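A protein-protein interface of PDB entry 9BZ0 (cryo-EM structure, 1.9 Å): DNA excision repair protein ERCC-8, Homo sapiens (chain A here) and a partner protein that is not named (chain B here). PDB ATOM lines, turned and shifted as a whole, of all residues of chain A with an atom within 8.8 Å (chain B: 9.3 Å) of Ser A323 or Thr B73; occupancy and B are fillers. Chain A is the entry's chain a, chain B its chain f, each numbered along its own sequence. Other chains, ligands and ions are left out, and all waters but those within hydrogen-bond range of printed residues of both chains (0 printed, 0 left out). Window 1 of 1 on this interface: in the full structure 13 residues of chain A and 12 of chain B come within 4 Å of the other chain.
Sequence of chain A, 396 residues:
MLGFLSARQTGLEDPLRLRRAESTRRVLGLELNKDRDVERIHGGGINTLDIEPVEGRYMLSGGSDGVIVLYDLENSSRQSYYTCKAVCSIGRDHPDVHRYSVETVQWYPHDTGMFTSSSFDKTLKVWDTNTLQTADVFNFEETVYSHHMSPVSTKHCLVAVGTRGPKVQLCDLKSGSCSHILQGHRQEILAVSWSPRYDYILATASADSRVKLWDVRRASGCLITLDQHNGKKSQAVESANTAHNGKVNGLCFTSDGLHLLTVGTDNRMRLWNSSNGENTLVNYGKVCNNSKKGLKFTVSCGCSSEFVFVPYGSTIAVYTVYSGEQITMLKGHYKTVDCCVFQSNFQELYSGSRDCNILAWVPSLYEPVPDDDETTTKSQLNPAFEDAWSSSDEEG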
ATOM      1  N   MET A 269      -3.899  18.810  -5.158  1.00  0.00           N
ATOM      2  CA  MET A 269      -3.070  17.741  -4.625  1.00  0.00           C
ATOM      3  C   MET A 269      -2.355  18.268  -3.391  1.00  0.00           C
ATOM      4  O   MET A 269      -1.862  19.396  -3.396  1.00  0.00           O
ATOM      5  CB  MET A 269      -2.095  17.232  -5.686  1.00  0.00           C
ATOM      6  CG  MET A 269      -1.222  16.082  -5.249  1.00  0.00           C
ATOM      7  SD  MET A 269      -0.470  15.238  -6.640  1.00  0.00           S
ATOM      8  CE  MET A 269       0.575  16.520  -7.294  1.00  0.00           C
ATOM      9  N   LEU A 271       0.383  17.259   0.019  1.00  0.00           N
ATOM     10  CA  LEU A 271       1.432  16.426   0.592  1.00  0.00           C
ATOM     11  C   LEU A 271       1.379  16.465   2.112  1.00  0.00           C
ATOM     12  O   LEU A 271       1.266  17.537   2.703  1.00  0.00           O
ATOM     13  CB  LEU A 271       2.794  16.893   0.093  1.00  0.00           C
ATOM     14  CG  LEU A 271       4.045  16.114   0.464  1.00  0.00           C
ATOM     15  CD1 LEU A 271       4.072  14.791  -0.247  1.00  0.00           C
ATOM     16  CD2 LEU A 271       5.256  16.928   0.101  1.00  0.00           C
ATOM     17  N   THR A 280       2.191  19.541   4.588  1.00  0.00           N
ATOM     18  CA  THR A 280       3.493  20.120   4.298  1.00  0.00           C
ATOM     19  C   THR A 280       3.400  21.440   3.536  1.00  0.00           C
ATOM     20  O   THR A 280       4.418  22.111   3.366  1.00  0.00           O
ATOM     21  CB  THR A 280       4.302  19.077   3.518  1.00  0.00           C
ATOM     22  OG1 THR A 280       4.386  17.890   4.309  1.00  0.00           O
ATOM     23  CG2 THR A 280       5.713  19.533   3.233  1.00  0.00           C
ATOM     24  N   LEU A 281       2.204  21.872   3.155  1.00  0.00           N
ATOM     25  CA  LEU A 281       1.960  23.153   2.491  1.00  0.00           C
ATOM     26  C   LEU A 281       2.620  23.284   1.123  1.00  0.00           C
ATOM     27  O   LEU A 281       2.786  24.399   0.628  1.00  0.00           O
ATOM     28  CB  LEU A 281       2.364  24.336   3.375  1.00  0.00           C
ATOM     29  CG  LEU A 281       1.775  24.345   4.776  1.00  0.00           C
ATOM     30  CD1 LEU A 281       2.285  25.535   5.544  1.00  0.00           C
ATOM     31  CD2 LEU A 281       0.281  24.391   4.685  1.00  0.00           C
ATOM     32  N   VAL A 282       3.010  22.191   0.481  1.00  0.00           N
ATOM     33  CA  VAL A 282       3.404  22.267  -0.918  1.00  0.00           C
ATOM     34  C   VAL A 282       2.164  22.556  -1.749  1.00  0.00           C
ATOM     35  O   VAL A 282       1.104  21.960  -1.529  1.00  0.00           O
ATOM     36  CB  VAL A 282       4.107  20.978  -1.360  1.00  0.00           C
ATOM     37  CG1 VAL A 282       4.613  21.120  -2.766  1.00  0.00           C
ATOM     38  CG2 VAL A 282       5.255  20.690  -0.436  1.00  0.00           C
ATOM     39  N   ASN A 283       2.277  23.477  -2.696  1.00  0.00           N
ATOM     40  CA  ASN A 283       1.146  23.877  -3.520  1.00  0.00           C
ATOM     41  C   ASN A 283       1.451  23.620  -4.985  1.00  0.00           C
ATOM     42  O   ASN A 283       2.419  24.157  -5.525  1.00  0.00           O
ATOM     43  CB  ASN A 283       0.840  25.356  -3.287  1.00  0.00           C
ATOM     44  CG  ASN A 283      -0.451  25.796  -3.907  1.00  0.00           C
ATOM     45  OD1 ASN A 283      -0.884  25.271  -4.924  1.00  0.00           O
ATOM     46  ND2 ASN A 283      -1.077  26.785  -3.298  1.00  0.00           N
ATOM     47  N   TYR A 284       0.623  22.803  -5.619  1.00  0.00           N
ATOM     48  CA  TYR A 284       0.820  22.386  -6.993  1.00  0.00           C
ATOM     49  C   TYR A 284      -0.046  23.142  -7.984  1.00  0.00           C
ATOM     50  O   TYR A 284       0.062  22.901  -9.186  1.00  0.00           O
ATOM     51  CB  TYR A 284       0.564  20.887  -7.128  1.00  0.00           C
ATOM     52  CG  TYR A 284       1.372  20.042  -6.190  1.00  0.00           C
ATOM     53  CD1 TYR A 284       2.658  19.677  -6.499  1.00  0.00           C
ATOM     54  CD2 TYR A 284       0.845  19.600  -5.002  1.00  0.00           C
ATOM     55  CE1 TYR A 284       3.386  18.902  -5.671  1.00  0.00           C
ATOM     56  CE2 TYR A 284       1.578  18.826  -4.156  1.00  0.00           C
ATOM     57  CZ  TYR A 284       2.847  18.480  -4.497  1.00  0.00           C
ATOM     58  OH  TYR A 284       3.592  17.718  -3.643  1.00  0.00           O
ATOM     59  N   GLY A 285      -0.880  24.053  -7.524  1.00  0.00           N
ATOM     60  CA  GLY A 285      -1.852  24.688  -8.383  1.00  0.00           C
ATOM     61  C   GLY A 285      -3.105  23.857  -8.585  1.00  0.00           C
ATOM     62  O   GLY A 285      -3.429  22.972  -7.800  1.00  0.00           O
ATOM     63  N   SER A 305      15.412  13.920  -8.374  1.00  0.00           N
ATOM     64  CA  SER A 305      14.163  14.457  -7.863  1.00  0.00           C
ATOM     65  C   SER A 305      13.115  13.359  -7.802  1.00  0.00           C
ATOM     66  O   SER A 305      13.026  12.528  -8.706  1.00  0.00           O
ATOM     67  CB  SER A 305      13.672  15.604  -8.739  1.00  0.00           C
ATOM     68  OG  SER A 305      14.539  16.716  -8.638  1.00  0.00           O
ATOM     69  N   GLU A 306      12.318  13.353  -6.743  1.00  0.00           N
ATOM     70  CA  GLU A 306      11.122  12.526  -6.725  1.00  0.00           C
ATOM     71  C   GLU A 306      10.009  13.215  -7.503  1.00  0.00           C
ATOM     72  O   GLU A 306       9.562  14.297  -7.121  1.00  0.00           O
ATOM     73  CB  GLU A 306      10.683  12.253  -5.293  1.00  0.00           C
ATOM     74  CG  GLU A 306       9.581  11.218  -5.193  1.00  0.00           C
ATOM     75  CD  GLU A 306       9.442  10.634  -3.802  1.00  0.00           C
ATOM     76  OE1 GLU A 306       9.726  11.354  -2.821  1.00  0.00           O
ATOM     77  OE2 GLU A 306       9.048   9.456  -3.689  1.00  0.00           O
ATOM     78  N   TYR A 319       4.957  16.548 -11.693  1.00  0.00           N
ATOM     79  CA  TYR A 319       5.412  17.517 -10.709  1.00  0.00           C
ATOM     80  C   TYR A 319       6.638  17.019  -9.964  1.00  0.00           C
ATOM     81  O   TYR A 319       6.830  15.818  -9.789  1.00  0.00           O
ATOM     82  CB  TYR A 319       4.327  17.834  -9.679  1.00  0.00           C
ATOM     83  CG  TYR A 319       3.090  18.446 -10.248  1.00  0.00           C
ATOM     84  CD1 TYR A 319       2.066  17.661 -10.729  1.00  0.00           C
ATOM     85  CD2 TYR A 319       2.938  19.813 -10.289  1.00  0.00           C
ATOM     86  CE1 TYR A 319       0.924  18.218 -11.201  1.00  0.00           C
ATOM     87  CE2 TYR A 319       1.815  20.380 -10.802  1.00  0.00           C
ATOM     88  CZ  TYR A 319       0.803  19.578 -11.248  1.00  0.00           C
ATOM     89  OH  TYR A 319      -0.313  20.137 -11.804  1.00  0.00           O
ATOM     90  N   THR A 320       7.468  17.960  -9.528  1.00  0.00           N
ATOM     91  CA  THR A 320       8.424  17.699  -8.461  1.00  0.00           C
ATOM     92  C   THR A 320       7.709  17.734  -7.120  1.00  0.00           C
ATOM     93  O   THR A 320       7.102  18.742  -6.762  1.00  0.00           O
ATOM     94  CB  THR A 320       9.553  18.715  -8.484  1.00  0.00           C
ATOM     95  OG1 THR A 320       9.003  20.034  -8.516  1.00  0.00           O
ATOM     96  CG2 THR A 320      10.402  18.518  -9.701  1.00  0.00           C
ATOM     97  N   VAL A 321       7.806  16.632  -6.381  1.00  0.00           N
ATOM     98  CA  VAL A 321       6.985  16.424  -5.194  1.00  0.00           C
ATOM     99  C   VAL A 321       7.233  17.511  -4.159  1.00  0.00           C
ATOM    100  O   VAL A 321       6.298  18.121  -3.637  1.00  0.00           O
ATOM    101  CB  VAL A 321       7.254  15.028  -4.608  1.00  0.00           C
ATOM    102  CG1 VAL A 321       6.578  14.872  -3.284  1.00  0.00           C
ATOM    103  CG2 VAL A 321       6.779  13.968  -5.538  1.00  0.00           C
ATOM    104  N   TYR A 322       8.494  17.778  -3.855  1.00  0.00           N
ATOM    105  CA  TYR A 322       8.797  18.719  -2.786  1.00  0.00           C
ATOM    106  C   TYR A 322       8.758  20.171  -3.237  1.00  0.00           C
ATOM    107  O   TYR A 322       8.398  21.041  -2.445  1.00  0.00           O
ATOM    108  CB  TYR A 322      10.148  18.374  -2.187  1.00  0.00           C
ATOM    109  CG  TYR A 322      10.158  16.958  -1.718  1.00  0.00           C
ATOM    110  CD1 TYR A 322       9.336  16.549  -0.691  1.00  0.00           C
ATOM    111  CD2 TYR A 322      10.925  16.012  -2.353  1.00  0.00           C
ATOM    112  CE1 TYR A 322       9.329  15.256  -0.273  1.00  0.00           C
ATOM    113  CE2 TYR A 322      10.914  14.715  -1.953  1.00  0.00           C
ATOM    114  CZ  TYR A 322      10.119  14.341  -0.910  1.00  0.00           C
ATOM    115  OH  TYR A 322      10.087  13.032  -0.515  1.00  0.00           O
ATOM    116  N   SER A 323       9.115  20.457  -4.480  1.00  0.00           N
ATOM    117  CA  SER A 323       9.121  21.828  -4.955  1.00  0.00           C
ATOM    118  C   SER A 323       7.779  22.307  -5.478  1.00  0.00           C
ATOM    119  O   SER A 323       7.599  23.510  -5.662  1.00  0.00           O
ATOM    120  CB  SER A 323      10.162  21.999  -6.057  1.00  0.00           C
ATOM    121  OG  SER A 323      11.436  21.578  -5.616  1.00  0.00           O
ATOM    122  N   GLY A 324       6.851  21.414  -5.759  1.00  0.00           N
ATOM    123  CA  GLY A 324       5.590  21.833  -6.305  1.00  0.00           C
ATOM    124  C   GLY A 324       5.625  22.212  -7.761  1.00  0.00           C
ATOM    125  O   GLY A 324       4.573  22.528  -8.322  1.00  0.00           O
ATOM    126  N   GLU A 325       6.791  22.197  -8.390  1.00  0.00           N
ATOM    127  CA  GLU A 325       6.928  22.706  -9.745  1.00  0.00           C
ATOM    128  C   GLU A 325       6.333  21.737 -10.743  1.00  0.00           C
ATOM    129  O   GLU A 325       6.621  20.541 -10.708  1.00  0.00           O
ATOM    130  CB  GLU A 325       8.398  22.951 -10.061  1.00  0.00           C
ATOM    131  CG  GLU A 325       8.647  23.482 -11.455  1.00  0.00           C
ATOM    132  CD  GLU A 325      10.045  24.041 -11.627  1.00  0.00           C
ATOM    133  OE1 GLU A 325      10.983  23.510 -10.995  1.00  0.00           O
ATOM    134  OE2 GLU A 325      10.208  25.011 -12.397  1.00  0.00           O
ATOM    135  N   GLN A 326       5.492  22.252 -11.628  1.00  0.00           N
ATOM    136  CA  GLN A 326       4.990  21.477 -12.754  1.00  0.00           C
ATOM    137  C   GLN A 326       6.050  21.363 -13.838  1.00  0.00           C
ATOM    138  O   GLN A 326       6.561  22.373 -14.326  1.00  0.00           O
ATOM    139  CB  GLN A 326       3.725  22.104 -13.325  1.00  0.00           C
ATOM    140  CG  GLN A 326       3.029  21.209 -14.323  1.00  0.00           C
ATOM    141  CD  GLN A 326       1.657  21.695 -14.699  1.00  0.00           C
ATOM    142  OE1 GLN A 326       0.788  21.862 -13.848  1.00  0.00           O
ATOM    143  NE2 GLN A 326       1.447  21.918 -15.985  1.00  0.00           N
ATOM    144  N   ILE A 327       6.383  20.134 -14.208  1.00  0.00           N
ATOM    145  CA  ILE A 327       7.476  19.857 -15.123  1.00  0.00           C
ATOM    146  C   ILE A 327       6.989  19.691 -16.554  1.00  0.00           C
ATOM    147  O   ILE A 327       7.534  20.301 -17.471  1.00  0.00           O
ATOM    148  CB  ILE A 327       8.252  18.610 -14.651  1.00  0.00           C
ATOM    149  CG1 ILE A 327       8.980  18.887 -13.341  1.00  0.00           C
ATOM    150  CG2 ILE A 327       9.201  18.162 -15.709  1.00  0.00           C
ATOM    151  CD1 ILE A 327      10.049  19.920 -13.450  1.00  0.00           C
ATOM    152  N   PHE B  13      20.563  18.084 -14.286  1.00  0.00           N
ATOM    153  CA  PHE B  13      19.281  18.123 -14.977  1.00  0.00           C
ATOM    154  C   PHE B  13      19.230  19.356 -15.865  1.00  0.00           C
ATOM    155  O   PHE B  13      19.963  20.327 -15.657  1.00  0.00           O
ATOM    156  CB  PHE B  13      18.108  18.118 -13.990  1.00  0.00           C
ATOM    157  CG  PHE B  13      18.361  18.914 -12.740  1.00  0.00           C
ATOM    158  CD1 PHE B  13      18.445  20.297 -12.785  1.00  0.00           C
ATOM    159  CD2 PHE B  13      18.515  18.280 -11.518  1.00  0.00           C
ATOM    160  CE1 PHE B  13      18.677  21.030 -11.638  1.00  0.00           C
ATOM    161  CE2 PHE B  13      18.747  19.008 -10.367  1.00  0.00           C
ATOM    162  CZ  PHE B  13      18.828  20.385 -10.427  1.00  0.00           C
ATOM    163  N   VAL B  15      16.674  21.364 -16.089  1.00  0.00           N
ATOM    164  CA  VAL B  15      15.773  22.370 -15.539  1.00  0.00           C
ATOM    165  C   VAL B  15      16.567  23.556 -15.006  1.00  0.00           C
ATOM    166  O   VAL B  15      17.350  23.418 -14.066  1.00  0.00           O
ATOM    167  CB  VAL B  15      14.879  21.774 -14.438  1.00  0.00           C
ATOM    168  CG1 VAL B  15      13.926  22.832 -13.901  1.00  0.00           C
ATOM    169  CG2 VAL B  15      14.112  20.575 -14.970  1.00  0.00           C
ATOM    170  N   ALA B  36       6.172  37.621   0.092  1.00  0.00           N
ATOM    171  CA  ALA B  36       4.739  37.724   0.329  1.00  0.00           C
ATOM    172  C   ALA B  36       4.377  38.998   1.073  1.00  0.00           C
ATOM    173  O   ALA B  36       3.294  39.546   0.862  1.00  0.00           O
ATOM    174  CB  ALA B  36       4.243  36.504   1.093  1.00  0.00           C
ATOM    175  N   ARG B  62      -5.777  35.736  -1.494  1.00  0.00           N
ATOM    176  CA  ARG B  62      -4.621  34.859  -1.608  1.00  0.00           C
ATOM    177  C   ARG B  62      -4.232  34.581  -3.047  1.00  0.00           C
ATOM    178  O   ARG B  62      -3.046  34.441  -3.356  1.00  0.00           O
ATOM    179  CB  ARG B  62      -4.919  33.562  -0.875  1.00  0.00           C
ATOM    180  CG  ARG B  62      -3.743  32.675  -0.635  1.00  0.00           C
ATOM    181  CD  ARG B  62      -4.228  31.386  -0.061  1.00  0.00           C
ATOM    182  NE  ARG B  62      -3.188  30.742   0.714  1.00  0.00           N
ATOM    183  CZ  ARG B  62      -3.261  30.559   2.022  1.00  0.00           C
ATOM    184  NH1 ARG B  62      -2.193  30.117   2.676  1.00  0.00           N
ATOM    185  NH2 ARG B  62      -4.389  30.743   2.680  1.00  0.00           N
ATOM    186  N   TYR B  66      -0.303  35.159  -5.356  1.00  0.00           N
ATOM    187  CA  TYR B  66       0.363  34.303  -6.331  1.00  0.00           C
ATOM    188  C   TYR B  66       0.604  34.958  -7.681  1.00  0.00           C
ATOM    189  O   TYR B  66       1.367  34.415  -8.480  1.00  0.00           O
ATOM    190  CB  TYR B  66      -0.416  33.023  -6.573  1.00  0.00           C
ATOM    191  CG  TYR B  66      -0.739  32.238  -5.354  1.00  0.00           C
ATOM    192  CD1 TYR B  66       0.174  32.109  -4.340  1.00  0.00           C
ATOM    193  CD2 TYR B  66      -1.934  31.570  -5.246  1.00  0.00           C
ATOM    194  CE1 TYR B  66      -0.110  31.378  -3.239  1.00  0.00           C
ATOM    195  CE2 TYR B  66      -2.223  30.832  -4.151  1.00  0.00           C
ATOM    196  CZ  TYR B  66      -1.310  30.740  -3.148  1.00  0.00           C
ATOM    197  OH  TYR B  66      -1.605  29.993  -2.040  1.00  0.00           O
ATOM    198  N   VAL B  69       3.963  36.588  -6.546  1.00  0.00           N
ATOM    199  CA  VAL B  69       4.932  35.611  -6.065  1.00  0.00           C
ATOM    200  C   VAL B  69       4.624  34.282  -6.738  1.00  0.00           C
ATOM    201  O   VAL B  69       3.885  33.460  -6.183  1.00  0.00           O
ATOM    202  CB  VAL B  69       4.881  35.477  -4.534  1.00  0.00           C
ATOM    203  CG1 VAL B  69       6.013  34.605  -4.041  1.00  0.00           C
ATOM    204  CG2 VAL B  69       4.912  36.831  -3.868  1.00  0.00           C
ATOM    205  N   PRO B  70       5.152  34.045  -7.935  1.00  0.00           N
ATOM    206  CA  PRO B  70       4.742  32.871  -8.721  1.00  0.00           C
ATOM    207  C   PRO B  70       5.004  31.513  -8.080  1.00  0.00           C
ATOM    208  O   PRO B  70       4.265  30.566  -8.372  1.00  0.00           O
ATOM    209  CB  PRO B  70       5.540  33.034 -10.021  1.00  0.00           C
ATOM    210  CG  PRO B  70       5.776  34.489 -10.127  1.00  0.00           C
ATOM    211  CD  PRO B  70       5.994  34.957  -8.717  1.00  0.00           C
ATOM    212  N   ASP B  71       6.017  31.369  -7.227  1.00  0.00           N
ATOM    213  CA  ASP B  71       6.219  30.118  -6.493  1.00  0.00           C
ATOM    214  C   ASP B  71       5.192  30.028  -5.373  1.00  0.00           C
ATOM    215  O   ASP B  71       5.367  30.601  -4.299  1.00  0.00           O
ATOM    216  CB  ASP B  71       7.643  30.041  -5.961  1.00  0.00           C
ATOM    217  CG  ASP B  71       7.965  28.700  -5.312  1.00  0.00           C
ATOM    218  OD1 ASP B  71       7.054  28.022  -4.795  1.00  0.00           O
ATOM    219  OD2 ASP B  71       9.153  28.319  -5.324  1.00  0.00           O
ATOM    220  N   ARG B  72       4.118  29.284  -5.635  1.00  0.00           N
ATOM    221  CA  ARG B  72       3.005  29.166  -4.704  1.00  0.00           C
ATOM    222  C   ARG B  72       3.399  28.563  -3.368  1.00  0.00           C
ATOM    223  O   ARG B  72       2.823  28.922  -2.339  1.00  0.00           O
ATOM    224  CB  ARG B  72       1.900  28.331  -5.327  1.00  0.00           C
ATOM    225  CG  ARG B  72       1.355  28.912  -6.575  1.00  0.00           C
ATOM    226  CD  ARG B  72       0.296  28.040  -7.147  1.00  0.00           C
ATOM    227  NE  ARG B  72      -0.154  28.588  -8.411  1.00  0.00           N
ATOM    228  CZ  ARG B  72      -1.246  29.322  -8.551  1.00  0.00           C
ATOM    229  NH1 ARG B  72      -1.470  29.939  -9.707  1.00  0.00           N
ATOM    230  NH2 ARG B  72      -2.140  29.418  -7.582  1.00  0.00           N
ATOM    231  N   THR B  73       4.376  27.664  -3.349  1.00  0.00           N
ATOM    232  CA  THR B  73       4.787  27.063  -2.089  1.00  0.00           C
ATOM    233  C   THR B  73       5.501  28.070  -1.203  1.00  0.00           C
ATOM    234  O   THR B  73       5.215  28.178  -0.006  1.00  0.00           O
ATOM    235  CB  THR B  73       5.675  25.850  -2.357  1.00  0.00           C
ATOM    236  OG1 THR B  73       4.943  24.881  -3.109  1.00  0.00           O
ATOM    237  CG2 THR B  73       6.109  25.221  -1.062  1.00  0.00           C
ATOM    238  N   VAL B  74       6.421  28.828  -1.784  1.00  0.00           N
ATOM    239  CA  VAL B  74       7.109  29.881  -1.052  1.00  0.00           C
ATOM    240  C   VAL B  74       6.131  30.944  -0.581  1.00  0.00           C
ATOM    241  O   VAL B  74       6.197  31.404   0.564  1.00  0.00           O
ATOM    242  CB  VAL B  74       8.209  30.478  -1.940  1.00  0.00           C
ATOM    243  CG1 VAL B  74       8.769  31.735  -1.319  1.00  0.00           C
ATOM    244  CG2 VAL B  74       9.287  29.459  -2.179  1.00  0.00           C
ATOM    245  N   ALA B  75       5.200  31.336  -1.444  1.00  0.00           N
ATOM    246  CA  ALA B  75       4.148  32.264  -1.051  1.00  0.00           C
ATOM    247  C   ALA B  75       3.337  31.759   0.132  1.00  0.00           C
ATOM    248  O   ALA B  75       3.131  32.487   1.105  1.00  0.00           O
ATOM    249  CB  ALA B  75       3.235  32.535  -2.240  1.00  0.00           C
ATOM    250  N   ASP B  76       2.859  30.525   0.070  1.00  0.00           N
ATOM    251  CA  ASP B  76       2.069  29.983   1.168  1.00  0.00           C
ATOM    252  C   ASP B  76       2.861  29.889   2.463  1.00  0.00           C
ATOM    253  O   ASP B  76       2.329  30.176   3.541  1.00  0.00           O
ATOM    254  CB  ASP B  76       1.539  28.607   0.783  1.00  0.00           C
ATOM    255  CG  ASP B  76       0.340  28.680  -0.131  1.00  0.00           C
ATOM    256  OD1 ASP B  76      -0.354  29.716  -0.129  1.00  0.00           O
ATOM    257  OD2 ASP B  76       0.089  27.697  -0.858  1.00  0.00           O
ATOM    258  N   ARG B  77       4.131  29.511   2.389  1.00  0.00           N
ATOM    259  CA  ARG B  77       4.932  29.392   3.602  1.00  0.00           C
ATOM    260  C   ARG B  77       5.249  30.744   4.213  1.00  0.00           C
ATOM    261  O   ARG B  77       5.194  30.910   5.440  1.00  0.00           O
ATOM    262  CB  ARG B  77       6.196  28.609   3.300  1.00  0.00           C
ATOM    263  CG  ARG B  77       5.885  27.140   3.149  1.00  0.00           C
ATOM    264  CD  ARG B  77       7.060  26.312   2.711  1.00  0.00           C
ATOM    265  NE  ARG B  77       6.698  24.902   2.687  1.00  0.00           N
ATOM    266  CZ  ARG B  77       7.432  23.948   2.135  1.00  0.00           C
ATOM    267  NH1 ARG B  77       7.000  22.693   2.176  1.00  0.00           N
ATOM    268  NH2 ARG B  77       8.582  24.219   1.543  1.00  0.00           N
ATOM    269  N   GLN B  78       5.515  31.739   3.379  1.00  0.00           N
ATOM    270  CA  GLN B  78       5.719  33.088   3.885  1.00  0.00           C
ATOM    271  C   GLN B  78       4.442  33.674   4.470  1.00  0.00           C
ATOM    272  O   GLN B  78       4.484  34.384   5.476  1.00  0.00           O
ATOM    273  CB  GLN B  78       6.242  33.956   2.752  1.00  0.00           C
ATOM    274  CG  GLN B  78       7.635  33.598   2.332  1.00  0.00           C
ATOM    275  CD  GLN B  78       8.186  34.532   1.300  1.00  0.00           C
ATOM    276  OE1 GLN B  78       7.523  35.480   0.895  1.00  0.00           O
ATOM    277  NE2 GLN B  78       9.408  34.279   0.868  1.00  0.00           N
ATOM    278  N   LEU B  79       3.296  33.388   3.862  1.00  0.00           N
ATOM    279  CA  LEU B  79       2.025  33.787   4.451  1.00  0.00           C
ATOM    280  C   LEU B  79       1.778  33.128   5.801  1.00  0.00           C
ATOM    281  O   LEU B  79       1.290  33.779   6.731  1.00  0.00           O
ATOM    282  CB  LEU B  79       0.887  33.469   3.489  1.00  0.00           C
ATOM    283  CG  LEU B  79       0.735  34.340   2.245  1.00  0.00           C
ATOM    284  CD1 LEU B  79      -0.329  33.777   1.342  1.00  0.00           C
ATOM    285  CD2 LEU B  79       0.388  35.740   2.631  1.00  0.00           C
ATOM    286  N   LYS B  80       2.062  31.835   5.923  1.00  0.00           N
ATOM    287  CA  LYS B  80       1.949  31.165   7.213  1.00  0.00           C
ATOM    288  C   LYS B  80       2.857  31.790   8.262  1.00  0.00           C
ATOM    289  O   LYS B  80       2.469  31.939   9.428  1.00  0.00           O
ATOM    290  CB  LYS B  80       2.230  29.681   7.039  1.00  0.00           C
ATOM    291  CG  LYS B  80       1.973  28.817   8.261  1.00  0.00           C
ATOM    292  CD  LYS B  80       3.218  28.624   9.113  1.00  0.00           C
ATOM    293  CE  LYS B  80       2.958  27.636  10.239  1.00  0.00           C
ATOM    294  NZ  LYS B  80       4.162  27.423  11.086  1.00  0.00           N
ATOM    295  N   GLU B  81       4.047  32.214   7.866  1.00  0.00           N
ATOM    296  CA  GLU B  81       4.921  32.902   8.810  1.00  0.00           C
ATOM    297  C   GLU B  81       4.422  34.294   9.177  1.00  0.00           C
ATOM    298  O   GLU B  81       4.605  34.732  10.315  1.00  0.00           O
ATOM    299  CB  GLU B  81       6.330  32.993   8.236  1.00  0.00           C
ATOM    300  CG  GLU B  81       7.066  31.663   8.175  1.00  0.00           C
ATOM    301  CD  GLU B  81       8.471  31.799   7.619  1.00  0.00           C
ATOM    302  OE1 GLU B  81       8.808  32.890   7.113  1.00  0.00           O
ATOM    303  OE2 GLU B  81       9.239  30.817   7.688  1.00  0.00           O
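Thr B73 touches Leu A281.
CA of Val A282 touches OG1 of Thr B73 (3.7 Å).
Val A282 touches Arg B77 (CG2 to NH1, 3.7 Å).
Asn A283 touches Arg B72.
Ser A323 touches Thr B73 (O to OG1, 3.9 Å).
Of the printed residues of chain B, Thr A280 touches Arg B77 (2.9 Å).
Of the printed residues of chain B, Val A282 touches Thr B73 and Arg B77.
Tyr A284 touches none of the printed residues of chain B.
Ser A323 touches one residue of chain B.
Glu A325 touches none of the printed residues of chain B.
Of chain A, only Leu A281, Val A282, Asn A283 and Ser A323 come within 4 Å of Thr B73.
Printed residues of chain A within 4 Å of Arg B77: Thr A280 (2.9 Å) and Val A282 (3.7 Å).
The nearest residue of chain B that does not touch Ser A323 is Asp B71 (4.6 Å).
The nearest printed residue of chain A that does not touch Tyr B66 is Gly A285 (7.5 Å).
O of Leu A271 is in hydrogen-bond range of N of Thr A280, at 2.9 Å.
The side-chain amide oxygen of Asn A283 is in hydrogen-bond range of the backbone NH of Gly A285 (2.9 Å).
The guanidinium group (NE) of Arg B62 sits at hydrogen-bond distance from the side-chain hydroxyl (OH) of Tyr B66 (3.3 Å).
NE of Arg B62 lies within salt-bridge range of OD1 of Asp B76, 3.1 Å away.
OD2 of Asp B76 lies close to OH of Tyr B66 (3.1 Å).
The backbone NH of Thr B73 is in hydrogen-bond range of the side-chain carboxylate of Asp B71.
O of Thr A280 sits at hydrogen-bond distance from NH1 of Arg B77.
The side-chain hydroxyl of Tyr B66 sits at hydrogen-bond distance from the side-chain amide nitrogen of Asn A283 (3.5 Å).
The side-chain hydroxyl of Thr B73 is in hydrogen-bond range of the backbone NH of Asn A283, 3.0 Å away.
The side-chain carboxylate (OD2) of Asp B76 sits at hydrogen-bond distance from the side-chain amide nitrogen (ND2) of Asn A283 (2.9 Å).
Hydrophobic or aromatic side chains of chain B within 4 Å of the printed part of chain A: Tyr B66.
Hydrophobic or aromatic side chains of chain A that line the printed part of chain B: Val A282.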
